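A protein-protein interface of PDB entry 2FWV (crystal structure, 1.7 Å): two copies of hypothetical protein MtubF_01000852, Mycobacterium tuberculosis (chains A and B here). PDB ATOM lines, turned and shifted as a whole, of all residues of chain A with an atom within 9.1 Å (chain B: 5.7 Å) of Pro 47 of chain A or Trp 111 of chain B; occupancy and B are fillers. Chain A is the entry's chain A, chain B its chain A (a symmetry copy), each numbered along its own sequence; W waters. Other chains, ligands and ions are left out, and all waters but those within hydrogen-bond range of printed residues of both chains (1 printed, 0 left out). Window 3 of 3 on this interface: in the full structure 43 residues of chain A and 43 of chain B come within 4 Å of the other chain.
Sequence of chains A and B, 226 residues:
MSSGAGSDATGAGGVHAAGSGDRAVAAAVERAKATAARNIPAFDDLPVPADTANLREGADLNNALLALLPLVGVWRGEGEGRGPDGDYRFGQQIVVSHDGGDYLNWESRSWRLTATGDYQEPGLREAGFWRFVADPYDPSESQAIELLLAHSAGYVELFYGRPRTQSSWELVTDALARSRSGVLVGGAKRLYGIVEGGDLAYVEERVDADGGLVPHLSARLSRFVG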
ATOM      1  N   PHE A  43     -36.577  -9.078  17.197  1.00  0.00           N
ATOM      2  CA  PHE A  43     -35.477  -9.080  16.244  1.00  0.00           C
ATOM      3  C   PHE A  43     -34.181  -9.445  16.973  1.00  0.00           C
ATOM      4  O   PHE A  43     -33.949  -8.968  18.077  1.00  0.00           O
ATOM      5  CB  PHE A  43     -35.321  -7.691  15.628  1.00  0.00           C
ATOM      6  CG  PHE A  43     -36.310  -7.404  14.526  1.00  0.00           C
ATOM      7  CD1 PHE A  43     -36.393  -8.225  13.417  1.00  0.00           C
ATOM      8  CD2 PHE A  43     -37.142  -6.294  14.617  1.00  0.00           C
ATOM      9  CE1 PHE A  43     -37.307  -7.940  12.355  1.00  0.00           C
ATOM     10  CE2 PHE A  43     -38.060  -5.994  13.586  1.00  0.00           C
ATOM     11  CZ  PHE A  43     -38.136  -6.809  12.463  1.00  0.00           C
ATOM     12  N   ASP A  44     -33.356 -10.264  16.325  1.00  0.00           N
ATOM     13  CA  ASP A  44     -32.101 -10.752  16.922  1.00  0.00           C
ATOM     14  C   ASP A  44     -30.890 -10.155  16.216  1.00  0.00           C
ATOM     15  O   ASP A  44     -29.770 -10.667  16.343  1.00  0.00           O
ATOM     16  CB  ASP A  44     -32.045 -12.303  16.891  1.00  0.00           C
ATOM     17  CG  ASP A  44     -31.814 -12.890  15.491  1.00  0.00           C
ATOM     18  OD1 ASP A  44     -31.602 -12.142  14.503  1.00  0.00           O
ATOM     19  OD2 ASP A  44     -31.833 -14.154  15.369  1.00  0.00           O
ATOM     20  N   ASP A  45     -31.099  -9.067  15.471  1.00  0.00           N
ATOM     21  CA  ASP A  45     -30.081  -8.633  14.512  1.00  0.00           C
ATOM     22  C   ASP A  45     -29.616  -7.182  14.691  1.00  0.00           C
ATOM     23  O   ASP A  45     -29.007  -6.615  13.772  1.00  0.00           O
ATOM     24  CB  ASP A  45     -30.520  -8.922  13.065  1.00  0.00           C
ATOM     25  CG  ASP A  45     -31.792  -8.179  12.674  1.00  0.00           C
ATOM     26  OD1 ASP A  45     -32.449  -7.637  13.585  1.00  0.00           O
ATOM     27  OD2 ASP A  45     -32.106  -8.126  11.464  1.00  0.00           O
ATOM     28  N   LEU A  46     -29.898  -6.596  15.855  1.00  0.00           N
ATOM     29  CA  LEU A  46     -29.522  -5.216  16.141  1.00  0.00           C
ATOM     30  C   LEU A  46     -28.268  -5.203  17.030  1.00  0.00           C
ATOM     31  O   LEU A  46     -27.989  -6.209  17.695  1.00  0.00           O
ATOM     32  CB  LEU A  46     -30.644  -4.462  16.854  1.00  0.00           C
ATOM     33  CG  LEU A  46     -31.944  -4.231  16.051  1.00  0.00           C
ATOM     34  CD1 LEU A  46     -33.009  -3.628  16.954  1.00  0.00           C
ATOM     35  CD2 LEU A  46     -31.661  -3.349  14.858  1.00  0.00           C
ATOM     36  N   PRO A  47     -27.534  -4.074  17.058  1.00  0.00           N
ATOM     37  CA  PRO A  47     -26.357  -3.982  17.953  1.00  0.00           C
ATOM     38  C   PRO A  47     -26.688  -3.735  19.428  1.00  0.00           C
ATOM     39  O   PRO A  47     -25.797  -3.856  20.278  1.00  0.00           O
ATOM     40  CB  PRO A  47     -25.563  -2.800  17.388  1.00  0.00           C
ATOM     41  CG  PRO A  47     -26.554  -1.970  16.686  1.00  0.00           C
ATOM     42  CD  PRO A  47     -27.691  -2.858  16.233  1.00  0.00           C
ATOM     43  N   VAL A  48     -27.940  -3.364  19.717  1.00  0.00           N
ATOM     44  CA  VAL A  48     -28.451  -3.259  21.088  1.00  0.00           C
ATOM     45  C   VAL A  48     -29.063  -4.606  21.497  1.00  0.00           C
ATOM     46  O   VAL A  48     -29.446  -5.405  20.644  1.00  0.00           O
ATOM     47  CB  VAL A  48     -29.489  -2.119  21.238  1.00  0.00           C
ATOM     48  CG1 VAL A  48     -28.797  -0.728  21.095  1.00  0.00           C
ATOM     49  CG2 VAL A  48     -30.651  -2.300  20.232  1.00  0.00           C
ATOM     50  N   PRO A  49     -29.143  -4.886  22.816  1.00  0.00           N
ATOM     51  CA  PRO A  49     -29.715  -6.162  23.235  1.00  0.00           C
ATOM     52  C   PRO A  49     -31.174  -6.322  22.811  1.00  0.00           C
ATOM     53  O   PRO A  49     -31.948  -5.331  22.847  1.00  0.00           O
ATOM     54  CB  PRO A  49     -29.607  -6.109  24.779  1.00  0.00           C
ATOM     55  CG  PRO A  49     -28.491  -5.154  25.014  1.00  0.00           C
ATOM     56  CD  PRO A  49     -28.689  -4.088  23.966  1.00  0.00           C
ATOM     57  N   ALA A  50     -31.536  -7.544  22.412  1.00  0.00           N
ATOM     58  CA  ALA A  50     -32.936  -7.887  22.105  1.00  0.00           C
ATOM     59  C   ALA A  50     -33.773  -7.707  23.359  1.00  0.00           C
ATOM     60  O   ALA A  50     -33.310  -8.003  24.478  1.00  0.00           O
ATOM     61  CB  ALA A  50     -33.083  -9.283  21.608  1.00  0.00           C
ATOM     62  N   ASP A  99     -34.279  -4.256  28.016  1.00  0.00           N
ATOM     63  CA  ASP A  99     -33.156  -4.337  27.085  1.00  0.00           C
ATOM     64  C   ASP A  99     -31.814  -4.093  27.786  1.00  0.00           C
ATOM     65  O   ASP A  99     -30.818  -3.758  27.104  1.00  0.00           O
ATOM     66  CB  ASP A  99     -33.385  -3.349  25.909  1.00  0.00           C
ATOM     67  CG  ASP A  99     -33.484  -1.887  26.370  1.00  0.00           C
ATOM     68  OD1 ASP A  99     -33.015  -1.535  27.485  1.00  0.00           O
ATOM     69  OD2 ASP A  99     -34.012  -1.064  25.579  1.00  0.00           O
ATOM     70  N   GLY B  77     -31.341   2.821  10.282  1.00  0.00           N
ATOM     71  CA  GLY B  77     -30.300   3.652   9.689  1.00  0.00           C
ATOM     72  C   GLY B  77     -29.520   4.366  10.732  1.00  0.00           C
ATOM     73  O   GLY B  77     -29.447   3.907  11.863  1.00  0.00           O
ATOM     74  N   ARG B  89     -22.809  10.780  16.275  1.00  0.00           N
ATOM     75  CA  ARG B  89     -23.532   9.818  15.433  1.00  0.00           C
ATOM     76  C   ARG B  89     -24.377   8.904  16.301  1.00  0.00           C
ATOM     77  O   ARG B  89     -24.034   8.607  17.461  1.00  0.00           O
ATOM     78  CB  ARG B  89     -22.564   8.967  14.627  1.00  0.00           C
ATOM     79  CG  ARG B  89     -21.664   9.817  13.732  1.00  0.00           C
ATOM     80  CD  ARG B  89     -20.542   8.981  13.141  1.00  0.00           C
ATOM     81  NE  ARG B  89     -21.035   7.967  12.213  1.00  0.00           N
ATOM     82  CZ  ARG B  89     -20.253   7.192  11.468  1.00  0.00           C
ATOM     83  NH1 ARG B  89     -18.928   7.302  11.541  1.00  0.00           N
ATOM     84  NH2 ARG B  89     -20.803   6.313  10.630  1.00  0.00           N
ATOM     85  N   PHE B  90     -25.472   8.422  15.714  1.00  0.00           N
ATOM     86  CA  PHE B  90     -26.259   7.385  16.374  1.00  0.00           C
ATOM     87  C   PHE B  90     -26.876   6.444  15.348  1.00  0.00           C
ATOM     88  O   PHE B  90     -27.022   6.805  14.176  1.00  0.00           O
ATOM     89  CB  PHE B  90     -27.338   8.010  17.287  1.00  0.00           C
ATOM     90  CG  PHE B  90     -28.356   8.834  16.569  1.00  0.00           C
ATOM     91  CD1 PHE B  90     -29.517   8.235  16.053  1.00  0.00           C
ATOM     92  CD2 PHE B  90     -28.202  10.216  16.466  1.00  0.00           C
ATOM     93  CE1 PHE B  90     -30.508   9.032  15.386  1.00  0.00           C
ATOM     94  CE2 PHE B  90     -29.173  11.023  15.832  1.00  0.00           C
ATOM     95  CZ  PHE B  90     -30.325  10.429  15.266  1.00  0.00           C
ATOM     96  N   GLY B  91     -27.211   5.228  15.776  1.00  0.00           N
ATOM     97  CA  GLY B  91     -28.008   4.345  14.947  1.00  0.00           C
ATOM     98  C   GLY B  91     -29.427   4.282  15.512  1.00  0.00           C
ATOM     99  O   GLY B  91     -29.673   4.658  16.651  1.00  0.00           O
ATOM    100  N   GLN B  92     -30.356   3.839  14.686  1.00  0.00           N
ATOM    101  CA  GLN B  92     -31.763   3.854  15.105  1.00  0.00           C
ATOM    102  C   GLN B  92     -32.592   2.833  14.343  1.00  0.00           C
ATOM    103  O   GLN B  92     -32.347   2.576  13.137  1.00  0.00           O
ATOM    104  CB  GLN B  92     -32.303   5.255  14.814  1.00  0.00           C
ATOM    105  CG  GLN B  92     -33.737   5.483  15.262  1.00  0.00           C
ATOM    106  CD  GLN B  92     -34.156   6.927  15.130  1.00  0.00           C
ATOM    107  OE1 GLN B  92     -35.100   7.372  15.799  1.00  0.00           O
ATOM    108  NE2 GLN B  92     -33.499   7.658  14.273  1.00  0.00           N
ATOM    109  N   GLN B  93     -33.576   2.259  15.043  1.00  0.00           N
ATOM    110  CA  GLN B  93     -34.645   1.478  14.406  1.00  0.00           C
ATOM    111  C   GLN B  93     -35.965   2.067  14.834  1.00  0.00           C
ATOM    112  O   GLN B  93     -36.180   2.286  16.020  1.00  0.00           O
ATOM    113  CB  GLN B  93     -34.626   0.015  14.856  1.00  0.00           C
ATOM    114  CG  GLN B  93     -35.769  -0.805  14.251  1.00  0.00           C
ATOM    115  CD  GLN B  93     -35.780  -2.257  14.710  1.00  0.00           C
ATOM    116  OE1 GLN B  93     -35.353  -3.151  13.968  1.00  0.00           O
ATOM    117  NE2 GLN B  93     -36.310  -2.517  15.913  1.00  0.00           N
ATOM    118  N   ARG B 109     -35.977   3.033  18.819  1.00  0.00           N
ATOM    119  CA  ARG B 109     -34.831   2.742  19.693  1.00  0.00           C
ATOM    120  C   ARG B 109     -33.601   3.297  18.997  1.00  0.00           C
ATOM    121  O   ARG B 109     -33.404   3.073  17.799  1.00  0.00           O
ATOM    122  CB  ARG B 109     -34.683   1.240  19.963  1.00  0.00           C
ATOM    123  CG  ARG B 109     -35.892   0.587  20.607  1.00  0.00           C
ATOM    124  CD  ARG B 109     -35.769  -0.932  20.544  1.00  0.00           C
ATOM    125  NE  ARG B 109     -34.626  -1.437  21.322  1.00  0.00           N
ATOM    126  CZ  ARG B 109     -34.361  -2.733  21.482  1.00  0.00           C
ATOM    127  NH1 ARG B 109     -35.130  -3.648  20.894  1.00  0.00           N
ATOM    128  NH2 ARG B 109     -33.316  -3.108  22.211  1.00  0.00           N
ATOM    129  N   SER B 110     -32.790   4.017  19.759  1.00  0.00           N
ATOM    130  CA  SER B 110     -31.526   4.504  19.204  1.00  0.00           C
ATOM    131  C   SER B 110     -30.331   4.046  20.025  1.00  0.00           C
ATOM    132  O   SER B 110     -30.481   3.620  21.169  1.00  0.00           O
ATOM    133  CB  SER B 110     -31.543   6.024  19.108  1.00  0.00           C
ATOM    134  OG  SER B 110     -31.403   6.684  20.347  1.00  0.00           O
ATOM    135  N   TRP B 111     -29.143   4.193  19.446  1.00  0.00           N
ATOM    136  CA  TRP B 111     -27.930   3.863  20.161  1.00  0.00           C
ATOM    137  C   TRP B 111     -26.828   4.791  19.707  1.00  0.00           C
ATOM    138  O   TRP B 111     -26.769   5.169  18.547  1.00  0.00           O
ATOM    139  CB  TRP B 111     -27.528   2.392  19.957  1.00  0.00           C
ATOM    140  CG  TRP B 111     -27.491   1.907  18.518  1.00  0.00           C
ATOM    141  CD1 TRP B 111     -26.414   1.903  17.661  1.00  0.00           C
ATOM    142  CD2 TRP B 111     -28.594   1.375  17.776  1.00  0.00           C
ATOM    143  NE1 TRP B 111     -26.781   1.376  16.438  1.00  0.00           N
ATOM    144  CE2 TRP B 111     -28.119   1.042  16.487  1.00  0.00           C
ATOM    145  CE3 TRP B 111     -29.944   1.125  18.091  1.00  0.00           C
ATOM    146  CZ2 TRP B 111     -28.954   0.491  15.497  1.00  0.00           C
ATOM    147  CZ3 TRP B 111     -30.779   0.583  17.100  1.00  0.00           C
ATOM    148  CH2 TRP B 111     -30.283   0.269  15.829  1.00  0.00           C
ATOM    149  N   ARG B 112     -25.949   5.133  20.638  1.00  0.00           N
ATOM    150  CA  ARG B 112     -24.822   5.988  20.314  1.00  0.00           C
ATOM    151  C   ARG B 112     -23.770   5.219  19.541  1.00  0.00           C
ATOM    152  O   ARG B 112     -23.483   4.033  19.826  1.00  0.00           O
ATOM    153  CB  ARG B 112     -24.189   6.544  21.582  1.00  0.00           C
ATOM    154  CG  ARG B 112     -25.162   7.324  22.450  1.00  0.00           C
ATOM    155  CD  ARG B 112     -25.553   8.645  21.855  1.00  0.00           C
ATOM    156  NE  ARG B 112     -24.441   9.592  21.867  1.00  0.00           N
ATOM    157  CZ  ARG B 112     -24.455  10.772  22.485  1.00  0.00           C
ATOM    158  NH1 ARG B 112     -25.534  11.180  23.159  1.00  0.00           N
ATOM    159  NH2 ARG B 112     -23.380  11.545  22.429  1.00  0.00           N
ATOM    160  N   LEU B 113     -23.196   5.916  18.567  1.00  0.00           N
ATOM    161  CA  LEU B 113     -22.055   5.388  17.828  1.00  0.00           C
ATOM    162  C   LEU B 113     -20.859   6.261  18.128  1.00  0.00           C
ATOM    163  O   LEU B 113     -21.006   7.452  18.384  1.00  0.00           O
ATOM    164  CB  LEU B 113     -22.335   5.411  16.336  1.00  0.00           C
ATOM    165  CG  LEU B 113     -23.500   4.576  15.793  1.00  0.00           C
ATOM    166  CD1 LEU B 113     -23.701   4.919  14.345  1.00  0.00           C
ATOM    167  CD2 LEU B 113     -23.293   3.094  15.962  1.00  0.00           C
ATOM    168  N   TYR B 119     -20.441   0.828  17.440  1.00  0.00           N
ATOM    169  CA  TYR B 119     -21.376   0.786  18.555  1.00  0.00           C
ATOM    170  C   TYR B 119     -20.732   1.282  19.858  1.00  0.00           C
ATOM    171  O   TYR B 119     -19.659   0.804  20.246  1.00  0.00           O
ATOM    172  CB  TYR B 119     -21.898  -0.642  18.715  1.00  0.00           C
ATOM    173  CG  TYR B 119     -22.894  -0.764  19.829  1.00  0.00           C
ATOM    174  CD1 TYR B 119     -24.221  -0.367  19.639  1.00  0.00           C
ATOM    175  CD2 TYR B 119     -22.519  -1.250  21.076  1.00  0.00           C
ATOM    176  CE1 TYR B 119     -25.138  -0.462  20.650  1.00  0.00           C
ATOM    177  CE2 TYR B 119     -23.438  -1.352  22.112  1.00  0.00           C
ATOM    178  CZ  TYR B 119     -24.756  -0.949  21.884  1.00  0.00           C
ATOM    179  OH  TYR B 119     -25.698  -1.035  22.879  1.00  0.00           O
ATOM    180  N   GLU B 121     -22.902   2.723  22.981  1.00  0.00           N
ATOM    181  CA  GLU B 121     -23.760   2.407  24.118  1.00  0.00           C
ATOM    182  C   GLU B 121     -25.217   2.632  23.699  1.00  0.00           C
ATOM    183  O   GLU B 121     -25.462   3.284  22.678  1.00  0.00           O
ATOM    184  CB  GLU B 121     -23.418   3.316  25.303  1.00  0.00           C
ATOM    185  CG  GLU B 121     -23.384   4.797  24.952  1.00  0.00           C
ATOM    186  CD  GLU B 121     -22.978   5.678  26.112  1.00  0.00           C
ATOM    187  OE1 GLU B 121     -23.586   5.572  27.194  1.00  0.00           O
ATOM    188  OE2 GLU B 121     -22.062   6.505  25.934  1.00  0.00           O
ATOM    189  N   PRO B 122     -26.185   2.088  24.477  1.00  0.00           N
ATOM    190  CA  PRO B 122     -27.590   2.414  24.127  1.00  0.00           C
ATOM    191  C   PRO B 122     -27.927   3.896  24.229  1.00  0.00           C
ATOM    192  O   PRO B 122     -27.314   4.670  25.003  1.00  0.00           O
ATOM    193  CB  PRO B 122     -28.405   1.608  25.152  1.00  0.00           C
ATOM    194  CG  PRO B 122     -27.473   0.513  25.592  1.00  0.00           C
ATOM    195  CD  PRO B 122     -26.121   1.176  25.638  1.00  0.00           C
ATOM    196  N   GLY B 123     -28.883   4.279  23.393  1.00  0.00           N
ATOM    197  CA  GLY B 123     -29.390   5.616  23.389  1.00  0.00           C
ATOM    198  C   GLY B 123     -30.841   5.551  23.809  1.00  0.00           C
ATOM    199  O   GLY B 123     -31.251   4.669  24.546  1.00  0.00           O
ATOM    200  N   LEU B 124     -31.613   6.477  23.286  1.00  0.00           N
ATOM    201  CA  LEU B 124     -32.942   6.776  23.816  1.00  0.00           C
ATOM    202  C   LEU B 124     -33.975   5.873  23.202  1.00  0.00           C
ATOM    203  O   LEU B 124     -33.820   5.402  22.062  1.00  0.00           O
ATOM    204  CB  LEU B 124     -33.304   8.223  23.523  1.00  0.00           C
ATOM    205  CG  LEU B 124     -32.341   9.241  24.172  1.00  0.00           C
ATOM    206  CD1 LEU B 124     -32.643  10.584  23.585  1.00  0.00           C
ATOM    207  CD2 LEU B 124     -32.515   9.251  25.662  1.00  0.00           C
HETATM  208  O   HOH W   1     -33.169  -0.165  23.199  1.00  0.00           O
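O of Pro 49 of chain A sits at hydrogen-bond distance from NH2 of Arg 109 of chain B (2.7 Å).
N of Gly 91 of chain B is in hydrogen-bond range of O of Trp 111 of chain B (2.8 Å). The backbone NH (N) of Gln 93 of chain B is in hydrogen-bond range of the backbone carbonyl oxygen (O) of Arg 109 of chain B, at 2.9 Å.
Among the printed residues, merely in contact across the chains: Phe 43 of chain A with Gln 93 of chain B, Leu 46 of chain A with Gln 93 of chain B, Leu 46 of chain A with Trp 111 of chain B, Pro 47 of chain A with Trp 111 of chain B, Pro 47 of chain A with Tyr 119 of chain B, Val 48 of chain A with Arg 109 of chain B, Val 48 of chain A with Trp 111 of chain B, Val 48 of chain A with Tyr 119 of chain B and Asp 99 of chain A with Arg 109 of chain B.
Pro 47 of chain A touches just these residues of chain B: Trp 111 (3.4 Å) and Tyr 119 (3.5 Å). Printed residues of chain A within 4 Å of Trp 111 of chain B: Leu 46, Pro 47 and Val 48. No residue of chain A comes within 4 Å of Gly 91 of chain B. Printed residues of chain A within 4 Å of Tyr 119 of chain B: Pro 47 and Val 48. Of the printed residues of chain B, Val 48 of chain A touches Arg 109 (3.4 Å), Trp 111 (3.6 Å) and Tyr 119 (3.6 Å). Of the printed residues of chain B, Pro 49 of chain A touches Arg 109. Printed residues of chain B within 4 Å of Asp 99 of chain A: Arg 109. Of the printed residues of chain A, Arg 109 of chain B touches Val 48 (3.4 Å), Pro 49 (2.7 Å) and Asp 99 (3.7 Å).
Of the 9 printed residues of chain A, 6 touch a printed residue of chain B. Of the 16 printed residues of chain B, 4 touch a printed residue of chain A. Printed residues of chain B that touch a printed residue of chain A: Gln 93, Arg 109, Trp 111 and Tyr 119. Among the printed residues, 10 pairs touch across the chains.
No position is printed for both chains.
Water W1 bridges OD2 of Asp 99 of chain A and NE of Arg 109 of chain B.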
